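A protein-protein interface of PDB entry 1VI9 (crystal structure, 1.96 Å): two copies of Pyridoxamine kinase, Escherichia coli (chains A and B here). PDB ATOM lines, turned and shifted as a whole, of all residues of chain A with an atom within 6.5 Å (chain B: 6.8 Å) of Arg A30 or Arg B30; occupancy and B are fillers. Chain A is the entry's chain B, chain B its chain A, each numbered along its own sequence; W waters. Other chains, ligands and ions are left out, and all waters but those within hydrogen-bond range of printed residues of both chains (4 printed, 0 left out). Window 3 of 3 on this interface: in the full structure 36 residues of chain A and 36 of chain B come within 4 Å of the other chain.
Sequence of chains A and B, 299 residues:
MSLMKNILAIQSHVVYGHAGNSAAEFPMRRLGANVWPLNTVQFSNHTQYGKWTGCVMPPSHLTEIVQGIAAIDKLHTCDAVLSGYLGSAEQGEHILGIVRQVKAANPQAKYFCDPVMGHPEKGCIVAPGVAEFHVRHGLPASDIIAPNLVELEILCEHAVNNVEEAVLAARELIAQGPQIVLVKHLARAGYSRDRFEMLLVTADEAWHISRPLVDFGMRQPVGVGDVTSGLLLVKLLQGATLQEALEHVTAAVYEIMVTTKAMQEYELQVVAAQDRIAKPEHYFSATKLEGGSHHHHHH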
ATOM      1  N   GLU A  25       4.129 -21.114  26.872  1.00  0.00           N
ATOM      2  CA  GLU A  25       4.688 -19.901  27.481  1.00  0.00           C
ATOM      3  C   GLU A  25       5.982 -19.439  26.828  1.00  0.00           C
ATOM      4  O   GLU A  25       6.089 -18.245  26.514  1.00  0.00           O
ATOM      5  CB  GLU A  25       4.794 -20.072  28.991  1.00  0.00           C
ATOM      6  CG  GLU A  25       5.853 -19.261  29.717  1.00  0.00           C
ATOM      7  CD  GLU A  25       7.247 -19.840  29.655  1.00  0.00           C
ATOM      8  OE1 GLU A  25       7.383 -21.065  29.894  1.00  0.00           O
ATOM      9  OE2 GLU A  25       8.258 -19.149  29.377  1.00  0.00           O
ATOM     10  N   PHE A  26       6.943 -20.276  26.567  1.00  0.00           N
ATOM     11  CA  PHE A  26       8.220 -19.922  25.984  1.00  0.00           C
ATOM     12  C   PHE A  26       8.077 -19.379  24.570  1.00  0.00           C
ATOM     13  O   PHE A  26       8.529 -18.276  24.294  1.00  0.00           O
ATOM     14  CB  PHE A  26       9.246 -21.058  26.112  1.00  0.00           C
ATOM     15  CG  PHE A  26      10.509 -20.698  25.372  1.00  0.00           C
ATOM     16  CD1 PHE A  26      11.375 -19.784  25.924  1.00  0.00           C
ATOM     17  CD2 PHE A  26      10.769 -21.211  24.101  1.00  0.00           C
ATOM     18  CE1 PHE A  26      12.512 -19.396  25.222  1.00  0.00           C
ATOM     19  CE2 PHE A  26      11.912 -20.841  23.431  1.00  0.00           C
ATOM     20  CZ  PHE A  26      12.800 -19.920  23.991  1.00  0.00           C
ATOM     21  N   PRO A  27       7.349 -20.058  23.684  1.00  0.00           N
ATOM     22  CA  PRO A  27       7.135 -19.570  22.336  1.00  0.00           C
ATOM     23  C   PRO A  27       6.454 -18.215  22.334  1.00  0.00           C
ATOM     24  O   PRO A  27       6.797 -17.352  21.509  1.00  0.00           O
ATOM     25  CB  PRO A  27       6.347 -20.672  21.654  1.00  0.00           C
ATOM     26  CG  PRO A  27       6.748 -21.905  22.410  1.00  0.00           C
ATOM     27  CD  PRO A  27       6.849 -21.446  23.859  1.00  0.00           C
ATOM     28  N   MET A  28       5.461 -18.003  23.168  1.00  0.00           N
ATOM     29  CA  MET A  28       4.766 -16.740  23.308  1.00  0.00           C
ATOM     30  C   MET A  28       5.705 -15.636  23.800  1.00  0.00           C
ATOM     31  O   MET A  28       5.646 -14.518  23.265  1.00  0.00           O
ATOM     32  CB  MET A  28       3.591 -16.828  24.311  1.00  0.00           C
ATOM     33  CG  MET A  28       2.451 -17.685  23.716  1.00  0.00           C
ATOM     34  SD  MET A  28       1.192 -18.145  25.136  1.00  0.00           S
ATOM     35  CE  MET A  28       0.105 -16.623  24.995  1.00  0.00           C
ATOM     36  N   ARG A  29       6.528 -15.974  24.787  1.00  0.00           N
ATOM     37  CA  ARG A  29       7.492 -14.999  25.284  1.00  0.00           C
ATOM     38  C   ARG A  29       8.564 -14.785  24.215  1.00  0.00           C
ATOM     39  O   ARG A  29       9.013 -13.662  24.104  1.00  0.00           O
ATOM     40  CB  ARG A  29       8.135 -15.347  26.620  1.00  0.00           C
ATOM     41  CG  ARG A  29       7.154 -15.259  27.803  1.00  0.00           C
ATOM     42  CD  ARG A  29       7.793 -15.786  29.067  1.00  0.00           C
ATOM     43  NE  ARG A  29       6.975 -15.423  30.248  1.00  0.00           N
ATOM     44  CZ  ARG A  29       7.047 -16.093  31.398  1.00  0.00           C
ATOM     45  NH1 ARG A  29       7.864 -17.145  31.537  1.00  0.00           N
ATOM     46  NH2 ARG A  29       6.301 -15.705  32.437  1.00  0.00           N
ATOM     47  N   ARG A  30       8.956 -15.805  23.452  1.00  0.00           N
ATOM     48  CA  ARG A  30       9.912 -15.660  22.379  1.00  0.00           C
ATOM     49  C   ARG A  30       9.435 -14.700  21.298  1.00  0.00           C
ATOM     50  O   ARG A  30      10.248 -13.986  20.672  1.00  0.00           O
ATOM     51  CB  ARG A  30      10.338 -17.041  21.840  1.00  0.00           C
ATOM     52  CG  ARG A  30      11.530 -16.944  20.885  1.00  0.00           C
ATOM     53  CD  ARG A  30      12.834 -16.741  21.674  1.00  0.00           C
ATOM     54  NE  ARG A  30      13.945 -16.615  20.742  1.00  0.00           N
ATOM     55  CZ  ARG A  30      14.174 -15.614  19.917  1.00  0.00           C
ATOM     56  NH1 ARG A  30      13.394 -14.523  19.827  1.00  0.00           N
ATOM     57  NH2 ARG A  30      15.230 -15.713  19.107  1.00  0.00           N
ATOM     58  N   LEU A  31       8.151 -14.473  21.153  1.00  0.00           N
ATOM     59  CA  LEU A  31       7.572 -13.530  20.207  1.00  0.00           C
ATOM     60  C   LEU A  31       7.432 -12.136  20.792  1.00  0.00           C
ATOM     61  O   LEU A  31       6.880 -11.232  20.172  1.00  0.00           O
ATOM     62  CB  LEU A  31       6.214 -14.040  19.719  1.00  0.00           C
ATOM     63  CG  LEU A  31       6.187 -14.600  18.289  1.00  0.00           C
ATOM     64  CD1 LEU A  31       7.339 -15.514  18.002  1.00  0.00           C
ATOM     65  CD2 LEU A  31       4.848 -15.203  17.958  1.00  0.00           C
ATOM     66  N   GLY A  32       7.831 -11.951  22.065  1.00  0.00           N
ATOM     67  CA  GLY A  32       7.764 -10.622  22.637  1.00  0.00           C
ATOM     68  C   GLY A  32       6.554 -10.293  23.458  1.00  0.00           C
ATOM     69  O   GLY A  32       6.354  -9.107  23.752  1.00  0.00           O
ATOM     70  N   ALA A  33       5.758 -11.292  23.885  1.00  0.00           N
ATOM     71  CA  ALA A  33       4.614 -10.897  24.737  1.00  0.00           C
ATOM     72  C   ALA A  33       4.883 -11.407  26.165  1.00  0.00           C
ATOM     73  O   ALA A  33       5.717 -12.291  26.338  1.00  0.00           O
ATOM     74  CB  ALA A  33       3.336 -11.564  24.256  1.00  0.00           C
ATOM     75  N   VAL A 271      12.401 -25.052  22.704  1.00  0.00           N
ATOM     76  CA  VAL A 271      13.653 -24.368  23.017  1.00  0.00           C
ATOM     77  C   VAL A 271      14.601 -24.529  21.841  1.00  0.00           C
ATOM     78  O   VAL A 271      15.002 -23.528  21.231  1.00  0.00           O
ATOM     79  CB  VAL A 271      14.265 -24.777  24.345  1.00  0.00           C
ATOM     80  CG1 VAL A 271      15.618 -24.073  24.603  1.00  0.00           C
ATOM     81  CG2 VAL A 271      13.334 -24.418  25.513  1.00  0.00           C
ATOM     82  N   GLN A 274      13.651 -22.211  18.931  1.00  0.00           N
ATOM     83  CA  GLN A 274      13.273 -20.844  19.223  1.00  0.00           C
ATOM     84  C   GLN A 274      13.514 -19.798  18.174  1.00  0.00           C
ATOM     85  O   GLN A 274      12.653 -18.942  17.983  1.00  0.00           O
ATOM     86  CB  GLN A 274      13.842 -20.385  20.573  1.00  0.00           C
ATOM     87  CG  GLN A 274      15.376 -20.211  20.557  1.00  0.00           C
ATOM     88  CD  GLN A 274      15.772 -19.706  21.955  1.00  0.00           C
ATOM     89  OE1 GLN A 274      15.564 -18.542  22.255  1.00  0.00           O
ATOM     90  NE2 GLN A 274      16.258 -20.602  22.785  1.00  0.00           N
ATOM     91  N   ASP A 275      14.689 -19.791  17.522  1.00  0.00           N
ATOM     92  CA  ASP A 275      14.960 -18.775  16.512  1.00  0.00           C
ATOM     93  C   ASP A 275      13.992 -18.857  15.351  1.00  0.00           C
ATOM     94  O   ASP A 275      13.611 -17.827  14.792  1.00  0.00           O
ATOM     95  CB  ASP A 275      16.419 -18.862  16.048  1.00  0.00           C
ATOM     96  CG  ASP A 275      17.398 -18.418  17.104  1.00  0.00           C
ATOM     97  OD1 ASP A 275      17.012 -17.769  18.111  1.00  0.00           O
ATOM     98  OD2 ASP A 275      18.592 -18.723  16.974  1.00  0.00           O
ATOM     99  N   ARG A 276      13.527 -20.045  14.999  1.00  0.00           N
ATOM    100  CA  ARG A 276      12.596 -20.251  13.905  1.00  0.00           C
ATOM    101  C   ARG A 276      11.149 -20.074  14.271  1.00  0.00           C
ATOM    102  O   ARG A 276      10.244 -20.210  13.436  1.00  0.00           O
ATOM    103  CB  ARG A 276      12.921 -21.581  13.183  1.00  0.00           C
ATOM    104  CG  ARG A 276      14.255 -21.366  12.445  1.00  0.00           C
ATOM    105  CD  ARG A 276      14.945 -22.612  11.985  1.00  0.00           C
ATOM    106  NE  ARG A 276      14.944 -23.728  12.904  1.00  0.00           N
ATOM    107  CZ  ARG A 276      15.795 -23.964  13.881  1.00  0.00           C
ATOM    108  NH1 ARG A 276      16.809 -23.129  14.127  1.00  0.00           N
ATOM    109  NH2 ARG A 276      15.653 -25.042  14.634  1.00  0.00           N
ATOM    110  N   ILE A 277      10.879 -19.836  15.557  1.00  0.00           N
ATOM    111  CA  ILE A 277       9.526 -19.506  16.024  1.00  0.00           C
ATOM    112  C   ILE A 277       9.372 -18.005  15.746  1.00  0.00           C
ATOM    113  O   ILE A 277       8.434 -17.494  15.153  1.00  0.00           O
ATOM    114  CB  ILE A 277       9.407 -19.762  17.545  1.00  0.00           C
ATOM    115  CG1 ILE A 277       9.456 -21.258  17.797  1.00  0.00           C
ATOM    116  CG2 ILE A 277       8.134 -19.115  18.080  1.00  0.00           C
ATOM    117  CD1 ILE A 277       9.584 -21.747  19.215  1.00  0.00           C
ATOM    118  N   ALA A 278      10.426 -17.285  16.159  1.00  0.00           N
ATOM    119  CA  ALA A 278      10.431 -15.831  15.942  1.00  0.00           C
ATOM    120  C   ALA A 278      10.515 -15.550  14.442  1.00  0.00           C
ATOM    121  O   ALA A 278       9.824 -14.691  13.923  1.00  0.00           O
ATOM    122  CB  ALA A 278      11.637 -15.204  16.648  1.00  0.00           C
ATOM    123  N   LYS A 279      11.434 -16.207  13.759  1.00  0.00           N
ATOM    124  CA  LYS A 279      11.628 -15.987  12.317  1.00  0.00           C
ATOM    125  C   LYS A 279      11.702 -17.310  11.565  1.00  0.00           C
ATOM    126  O   LYS A 279      12.793 -17.875  11.424  1.00  0.00           O
ATOM    127  CB  LYS A 279      12.933 -15.245  12.042  1.00  0.00           C
ATOM    128  CG  LYS A 279      13.115 -13.869  12.653  1.00  0.00           C
ATOM    129  CD  LYS A 279      13.760 -13.934  14.034  1.00  0.00           C
ATOM    130  CE  LYS A 279      15.067 -14.749  13.976  1.00  0.00           C
ATOM    131  NZ  LYS A 279      15.340 -15.396  15.273  1.00  0.00           N
ATOM    132  N   GLU B  25      13.541 -19.245  34.524  1.00  0.00           N
ATOM    133  CA  GLU B  25      13.211 -20.121  33.419  1.00  0.00           C
ATOM    134  C   GLU B  25      13.374 -19.501  32.047  1.00  0.00           C
ATOM    135  O   GLU B  25      14.092 -20.100  31.229  1.00  0.00           O
ATOM    136  CB  GLU B  25      11.800 -20.762  33.592  1.00  0.00           C
ATOM    137  CG  GLU B  25      11.227 -21.257  32.253  1.00  0.00           C
ATOM    138  CD  GLU B  25      10.363 -20.262  31.513  1.00  0.00           C
ATOM    139  OE1 GLU B  25       9.611 -19.497  32.184  1.00  0.00           O
ATOM    140  OE2 GLU B  25      10.353 -20.185  30.236  1.00  0.00           O
ATOM    141  N   PHE B  26      12.748 -18.359  31.761  1.00  0.00           N
ATOM    142  CA  PHE B  26      12.849 -17.769  30.434  1.00  0.00           C
ATOM    143  C   PHE B  26      14.259 -17.452  30.023  1.00  0.00           C
ATOM    144  O   PHE B  26      14.692 -17.866  28.935  1.00  0.00           O
ATOM    145  CB  PHE B  26      11.809 -16.670  30.180  1.00  0.00           C
ATOM    146  CG  PHE B  26      11.974 -16.033  28.819  1.00  0.00           C
ATOM    147  CD1 PHE B  26      11.356 -16.585  27.706  1.00  0.00           C
ATOM    148  CD2 PHE B  26      12.758 -14.898  28.684  1.00  0.00           C
ATOM    149  CE1 PHE B  26      11.542 -15.992  26.464  1.00  0.00           C
ATOM    150  CE2 PHE B  26      12.946 -14.305  27.447  1.00  0.00           C
ATOM    151  CZ  PHE B  26      12.298 -14.846  26.334  1.00  0.00           C
ATOM    152  N   PRO B  27      15.062 -16.814  30.848  1.00  0.00           N
ATOM    153  CA  PRO B  27      16.455 -16.520  30.510  1.00  0.00           C
ATOM    154  C   PRO B  27      17.279 -17.744  30.201  1.00  0.00           C
ATOM    155  O   PRO B  27      18.075 -17.755  29.251  1.00  0.00           O
ATOM    156  CB  PRO B  27      16.961 -15.795  31.767  1.00  0.00           C
ATOM    157  CG  PRO B  27      15.737 -15.033  32.183  1.00  0.00           C
ATOM    158  CD  PRO B  27      14.650 -16.100  32.087  1.00  0.00           C
ATOM    159  N   MET B  28      17.124 -18.829  30.972  1.00  0.00           N
ATOM    160  CA  MET B  28      17.882 -20.062  30.718  1.00  0.00           C
ATOM    161  C   MET B  28      17.472 -20.696  29.382  1.00  0.00           C
ATOM    162  O   MET B  28      18.319 -21.229  28.660  1.00  0.00           O
ATOM    163  CB  MET B  28      17.624 -21.080  31.858  1.00  0.00           C
ATOM    164  CG  MET B  28      18.213 -20.642  33.187  1.00  0.00           C
ATOM    165  SD  MET B  28      17.940 -21.848  34.644  1.00  0.00           S
ATOM    166  CE  MET B  28      18.859 -23.379  34.119  1.00  0.00           C
ATOM    167  N   ARG B  29      16.153 -20.693  29.134  1.00  0.00           N
ATOM    168  CA  ARG B  29      15.653 -21.243  27.877  1.00  0.00           C
ATOM    169  C   ARG B  29      16.094 -20.359  26.709  1.00  0.00           C
ATOM    170  O   ARG B  29      16.409 -20.868  25.642  1.00  0.00           O
ATOM    171  CB  ARG B  29      14.134 -21.441  27.886  1.00  0.00           C
ATOM    172  CG  ARG B  29      13.653 -22.565  28.830  1.00  0.00           C
ATOM    173  CD  ARG B  29      12.111 -22.591  28.788  1.00  0.00           C
ATOM    174  NE  ARG B  29      11.586 -23.785  29.431  1.00  0.00           N
ATOM    175  CZ  ARG B  29      10.409 -23.959  29.999  1.00  0.00           C
ATOM    176  NH1 ARG B  29       9.508 -22.982  30.051  1.00  0.00           N
ATOM    177  NH2 ARG B  29      10.107 -25.161  30.488  1.00  0.00           N
ATOM    178  N   ARG B  30      16.217 -19.034  26.921  1.00  0.00           N
ATOM    179  CA  ARG B  30      16.626 -18.101  25.886  1.00  0.00           C
ATOM    180  C   ARG B  30      18.058 -18.364  25.444  1.00  0.00           C
ATOM    181  O   ARG B  30      18.371 -18.105  24.292  1.00  0.00           O
ATOM    182  CB  ARG B  30      16.388 -16.660  26.334  1.00  0.00           C
ATOM    183  CG  ARG B  30      16.481 -15.605  25.263  1.00  0.00           C
ATOM    184  CD  ARG B  30      15.429 -15.802  24.164  1.00  0.00           C
ATOM    185  NE  ARG B  30      15.632 -14.857  23.100  1.00  0.00           N
ATOM    186  CZ  ARG B  30      16.550 -14.915  22.136  1.00  0.00           C
ATOM    187  NH1 ARG B  30      17.399 -15.914  22.058  1.00  0.00           N
ATOM    188  NH2 ARG B  30      16.613 -13.914  21.261  1.00  0.00           N
ATOM    189  N   LEU B  31      18.899 -18.910  26.309  1.00  0.00           N
ATOM    190  CA  LEU B  31      20.241 -19.340  26.130  1.00  0.00           C
ATOM    191  C   LEU B  31      20.324 -20.758  25.530  1.00  0.00           C
ATOM    192  O   LEU B  31      21.430 -21.262  25.324  1.00  0.00           O
ATOM    193  CB  LEU B  31      21.062 -19.352  27.426  1.00  0.00           C
ATOM    194  CG  LEU B  31      21.535 -18.002  27.970  1.00  0.00           C
ATOM    195  CD1 LEU B  31      22.767 -18.172  28.869  1.00  0.00           C
ATOM    196  CD2 LEU B  31      21.813 -16.995  26.863  1.00  0.00           C
ATOM    197  N   GLY B  32      19.196 -21.484  25.414  1.00  0.00           N
ATOM    198  CA  GLY B  32      19.250 -22.789  24.780  1.00  0.00           C
ATOM    199  C   GLY B  32      19.252 -24.005  25.650  1.00  0.00           C
ATOM    200  O   GLY B  32      19.582 -25.127  25.183  1.00  0.00           O
ATOM    201  N   ALA B  33      18.984 -23.860  26.944  1.00  0.00           N
ATOM    202  CA  ALA B  33      18.954 -25.026  27.830  1.00  0.00           C
ATOM    203  C   ALA B  33      17.477 -25.342  28.132  1.00  0.00           C
ATOM    204  O   ALA B  33      16.618 -24.465  28.045  1.00  0.00           O
ATOM    205  CB  ALA B  33      19.677 -24.752  29.145  1.00  0.00           C
ATOM    206  N   LEU B 231      21.595 -18.533  34.874  1.00  0.00           N
ATOM    207  CA  LEU B 231      22.407 -18.354  33.678  1.00  0.00           C
ATOM    208  C   LEU B 231      23.791 -18.953  33.842  1.00  0.00           C
ATOM    209  O   LEU B 231      24.336 -19.466  32.844  1.00  0.00           O
ATOM    210  CB  LEU B 231      22.446 -16.909  33.196  1.00  0.00           C
ATOM    211  CG  LEU B 231      21.100 -16.292  32.781  1.00  0.00           C
ATOM    212  CD1 LEU B 231      21.318 -14.808  32.443  1.00  0.00           C
ATOM    213  CD2 LEU B 231      20.513 -16.979  31.567  1.00  0.00           C
ATOM    214  N   VAL B 270      12.848  -9.506  31.898  1.00  0.00           N
ATOM    215  CA  VAL B 270      13.508 -10.613  31.244  1.00  0.00           C
ATOM    216  C   VAL B 270      13.006 -10.857  29.832  1.00  0.00           C
ATOM    217  O   VAL B 270      13.846 -11.209  28.979  1.00  0.00           O
ATOM    218  CB  VAL B 270      13.462 -11.919  32.042  1.00  0.00           C
ATOM    219  CG1 VAL B 270      14.092 -11.725  33.418  1.00  0.00           C
ATOM    220  CG2 VAL B 270      12.013 -12.424  32.142  1.00  0.00           C
ATOM    221  N   VAL B 271      11.718 -10.623  29.552  1.00  0.00           N
ATOM    222  CA  VAL B 271      11.247 -10.802  28.192  1.00  0.00           C
ATOM    223  C   VAL B 271      11.676  -9.615  27.311  1.00  0.00           C
ATOM    224  O   VAL B 271      12.122  -9.813  26.185  1.00  0.00           O
ATOM    225  CB  VAL B 271       9.743 -11.047  28.088  1.00  0.00           C
ATOM    226  CG1 VAL B 271       9.286 -11.209  26.634  1.00  0.00           C
ATOM    227  CG2 VAL B 271       9.342 -12.310  28.868  1.00  0.00           C
ATOM    228  N   ALA B 273      14.233  -7.672  27.501  1.00  0.00           N
ATOM    229  CA  ALA B 273      15.668  -7.713  27.263  1.00  0.00           C
ATOM    230  C   ALA B 273      16.185  -9.002  26.650  1.00  0.00           C
ATOM    231  O   ALA B 273      17.395  -9.122  26.479  1.00  0.00           O
ATOM    232  CB  ALA B 273      16.368  -7.493  28.627  1.00  0.00           C
ATOM    233  N   GLN B 274      15.315  -9.911  26.190  1.00  0.00           N
ATOM    234  CA  GLN B 274      15.710 -11.196  25.678  1.00  0.00           C
ATOM    235  C   GLN B 274      16.789 -11.269  24.636  1.00  0.00           C
ATOM    236  O   GLN B 274      17.676 -12.120  24.826  1.00  0.00           O
ATOM    237  CB  GLN B 274      14.477 -12.060  25.255  1.00  0.00           C
ATOM    238  CG  GLN B 274      14.013 -11.732  23.850  1.00  0.00           C
ATOM    239  CD  GLN B 274      12.766 -12.502  23.450  1.00  0.00           C
ATOM    240  OE1 GLN B 274      12.890 -13.606  22.909  1.00  0.00           O
ATOM    241  NE2 GLN B 274      11.578 -11.949  23.734  1.00  0.00           N
ATOM    242  N   ASP B 275      16.814 -10.498  23.564  1.00  0.00           N
ATOM    243  CA  ASP B 275      17.882 -10.560  22.581  1.00  0.00           C
ATOM    244  C   ASP B 275      19.236 -10.201  23.189  1.00  0.00           C
ATOM    245  O   ASP B 275      20.266 -10.791  22.868  1.00  0.00           O
ATOM    246  CB  ASP B 275      17.593  -9.620  21.393  1.00  0.00           C
ATOM    247  CG  ASP B 275      16.356 -10.067  20.637  1.00  0.00           C
ATOM    248  OD1 ASP B 275      15.741 -11.092  20.995  1.00  0.00           O
ATOM    249  OD2 ASP B 275      15.967  -9.388  19.667  1.00  0.00           O
ATOM    250  N   ARG B 276      19.223  -9.371  24.234  1.00  0.00           N
ATOM    251  CA  ARG B 276      20.470  -8.993  24.906  1.00  0.00           C
ATOM    252  C   ARG B 276      20.843  -9.961  25.996  1.00  0.00           C
ATOM    253  O   ARG B 276      21.851  -9.817  26.704  1.00  0.00           O
ATOM    254  CB  ARG B 276      20.430  -7.530  25.273  1.00  0.00           C
ATOM    255  CG  ARG B 276      20.641  -6.652  24.013  1.00  0.00           C
ATOM    256  CD  ARG B 276      20.227  -5.204  24.316  1.00  0.00           C
ATOM    257  NE  ARG B 276      18.801  -5.105  24.573  1.00  0.00           N
ATOM    258  CZ  ARG B 276      18.260  -4.791  25.742  1.00  0.00           C
ATOM    259  NH1 ARG B 276      19.012  -4.520  26.816  1.00  0.00           N
ATOM    260  NH2 ARG B 276      16.940  -4.719  25.858  1.00  0.00           N
ATOM    261  N   ILE B 277      19.958 -10.960  26.238  1.00  0.00           N
ATOM    262  CA  ILE B 277      20.341 -12.001  27.221  1.00  0.00           C
ATOM    263  C   ILE B 277      21.224 -12.984  26.414  1.00  0.00           C
ATOM    264  O   ILE B 277      22.300 -13.386  26.832  1.00  0.00           O
ATOM    265  CB  ILE B 277      19.140 -12.744  27.813  1.00  0.00           C
ATOM    266  CG1 ILE B 277      18.416 -11.872  28.840  1.00  0.00           C
ATOM    267  CG2 ILE B 277      19.609 -14.037  28.484  1.00  0.00           C
ATOM    268  CD1 ILE B 277      17.148 -12.458  29.442  1.00  0.00           C
ATOM    269  N   ALA B 278      20.726 -13.357  25.223  1.00  0.00           N
ATOM    270  CA  ALA B 278      21.432 -14.279  24.351  1.00  0.00           C
ATOM    271  C   ALA B 278      22.711 -13.625  23.812  1.00  0.00           C
ATOM    272  O   ALA B 278      23.766 -14.269  23.717  1.00  0.00           O
ATOM    273  CB  ALA B 278      20.553 -14.697  23.179  1.00  0.00           C
ATOM    274  N   LYS B 279      22.619 -12.337  23.487  1.00  0.00           N
ATOM    275  CA  LYS B 279      23.766 -11.619  22.910  1.00  0.00           C
ATOM    276  C   LYS B 279      23.869 -10.217  23.482  1.00  0.00           C
ATOM    277  O   LYS B 279      23.292  -9.249  22.967  1.00  0.00           O
ATOM    278  CB  LYS B 279      23.584 -11.551  21.403  1.00  0.00           C
ATOM    279  CG  LYS B 279      23.660 -12.821  20.601  1.00  0.00           C
ATOM    280  CD  LYS B 279      22.339 -13.513  20.340  1.00  0.00           C
ATOM    281  CE  LYS B 279      21.400 -12.765  19.427  1.00  0.00           C
ATOM    282  NZ  LYS B 279      20.287 -12.059  20.124  1.00  0.00           N
HETATM  283  O   HOH W   1       7.118 -22.859  27.786  1.00  0.00           O
HETATM  284  O   HOH W   2      18.922 -16.852  19.910  1.00  0.00           O
HETATM  285  O   HOH W   3       7.528 -18.183  34.261  1.00  0.00           O
HETATM  286  O   HOH W   4      13.645 -11.791  19.183  1.00  0.00           O
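Water W2 lies within hydrogen-bond range of the side-chain carboxylate (OD1) of Asp A275 and the guanidinium group (NH1) of Arg B30.
Water W1 lies within hydrogen-bond range of the side-chain carboxylate of Glu A25, the backbone NH of Phe A26 and the guanidinium group of Arg B29.
Water W4 bridges the guanidinium group of Arg A30 (2.8 Å) and the side-chain carboxylate of Asp B275 (2.9 Å).
Water W3 lies within hydrogen-bond range of NH1 of Arg A29 (2.9 Å) and OE1 of Glu B25 (3.2 Å).
The guanidinium group of Arg B29 is in salt-bridge range of the side-chain carboxylate of Glu B25 (2.9 Å).
The guanidinium group (NE) of Arg B30 sits at hydrogen-bond distance from the side-chain amide oxygen (OE1) of Gln B274, at 3.0 Å.
The side-chain carboxylate (OD1) of Asp B275 is in salt-bridge range of the guanidinium group (NH2) of Arg B30 (3.0 Å).
The side-chain amide nitrogen (NE2) of Gln B274 is in hydrogen-bond range of the backbone carbonyl oxygen (O) of Val B271 (3.3 Å).
O of Met A28 lies within hydrogen-bond range of N of Ala A33 (3.3 Å).
The guanidinium group (NH2) of Arg A30 is in salt-bridge range of the side-chain carboxylate (OD1) of Asp A275 (2.9 Å).
OE2 of Glu A25 sits close to OE2 of Glu B25 (2.5 Å).
OE1 of Glu B25 lies within salt-bridge range of NH1 of Arg A29, at 3.0 Å.
NH1 of Arg B29 lies within salt-bridge range of OE1 of Glu A25 (2.9 Å).
The backbone carbonyl oxygen (O) of Arg B29 is in hydrogen-bond range of the side-chain amide nitrogen (NE2) of Gln A274 (2.9 Å).
The guanidinium group of Arg B30 lies within hydrogen-bond range of the side-chain amide oxygen of Gln A274 (3.2 Å).
NE2 of Gln B274 sits at hydrogen-bond distance from O of Arg A29, at 3.1 Å.
The side-chain amide oxygen (OE1) of Gln B274 is in hydrogen-bond range of the guanidinium group (NH1) of Arg A30 (3.3 Å).
The guanidinium group (NH2) of Arg A30 lies close to the guanidinium group (NH2) of Arg B30 (3.1 Å).
Among the printed residues, merely in contact across the chains: Val A271 with Arg B29, Arg A29 with Phe B26, Arg A29 with Val B271, Val A271 with Ala B33, Phe A26 with Phe B26, Phe A26 with Arg B29, Ala A33 with Val B271, Val A271 with Gly B32 and Arg A30 with Phe B26.
Glu B25 touches its own counterpart, Glu A25.
Phe B26 touches its own counterpart, Phe A26.
Phe A26 touches Arg B29, and with the chains exchanged Arg A29 touches Phe B26.
Arg A30 touches Gln B274, and with the chains exchanged Gln A274 touches Arg B30.
Positions printed for both chains: 25, 26, 27, 28, 29, 30, 31, 32, 33, 271, 274, 275, 276, 277, 278 and 279.
Of the 17 pairs that touch across the chains among the printed residues, 15 have their exchanged pair printed and touching as well.
Hydrophobic or aromatic side chains of chain A that line the printed part of chain B: Phe A26 and Val A271.
Along chain A the printed residues that touch a printed residue of chain B span positions 25 to 274.
Of the 19 printed residues of chain B, 8 touch a printed residue of chain A.
Hydrophobic or aromatic side chains of chain B within 4 Å of the printed part of chain A: Phe B26 and Val B271.
Among the printed residues, Asp or Glu carboxylates within 4 Å of a Lys or Arg side-chain nitrogen of the other chain: Glu A25 with Arg B29 (2.9 Å) and Arg A29 with Glu B25 (3.0 Å).
Of chain B, only Phe B26 (3.97 Å), Arg B30 (3.1 Å) and Gln B274 (3.3 Å) come within 4 Å of Arg A30.
Arg B30 touches just these residues of chain A: Arg A30 and Gln A274.
Of the printed residues of chain A, Gln B274 touches Arg A29 and Arg A30.
Of the printed residues of chain B, Ala A33 touches Val B271.
Lys B279 touches none of the printed residues of chain A.
The nearest residue of chain A that does not touch Arg B30 is Phe A26 (4.1 Å).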
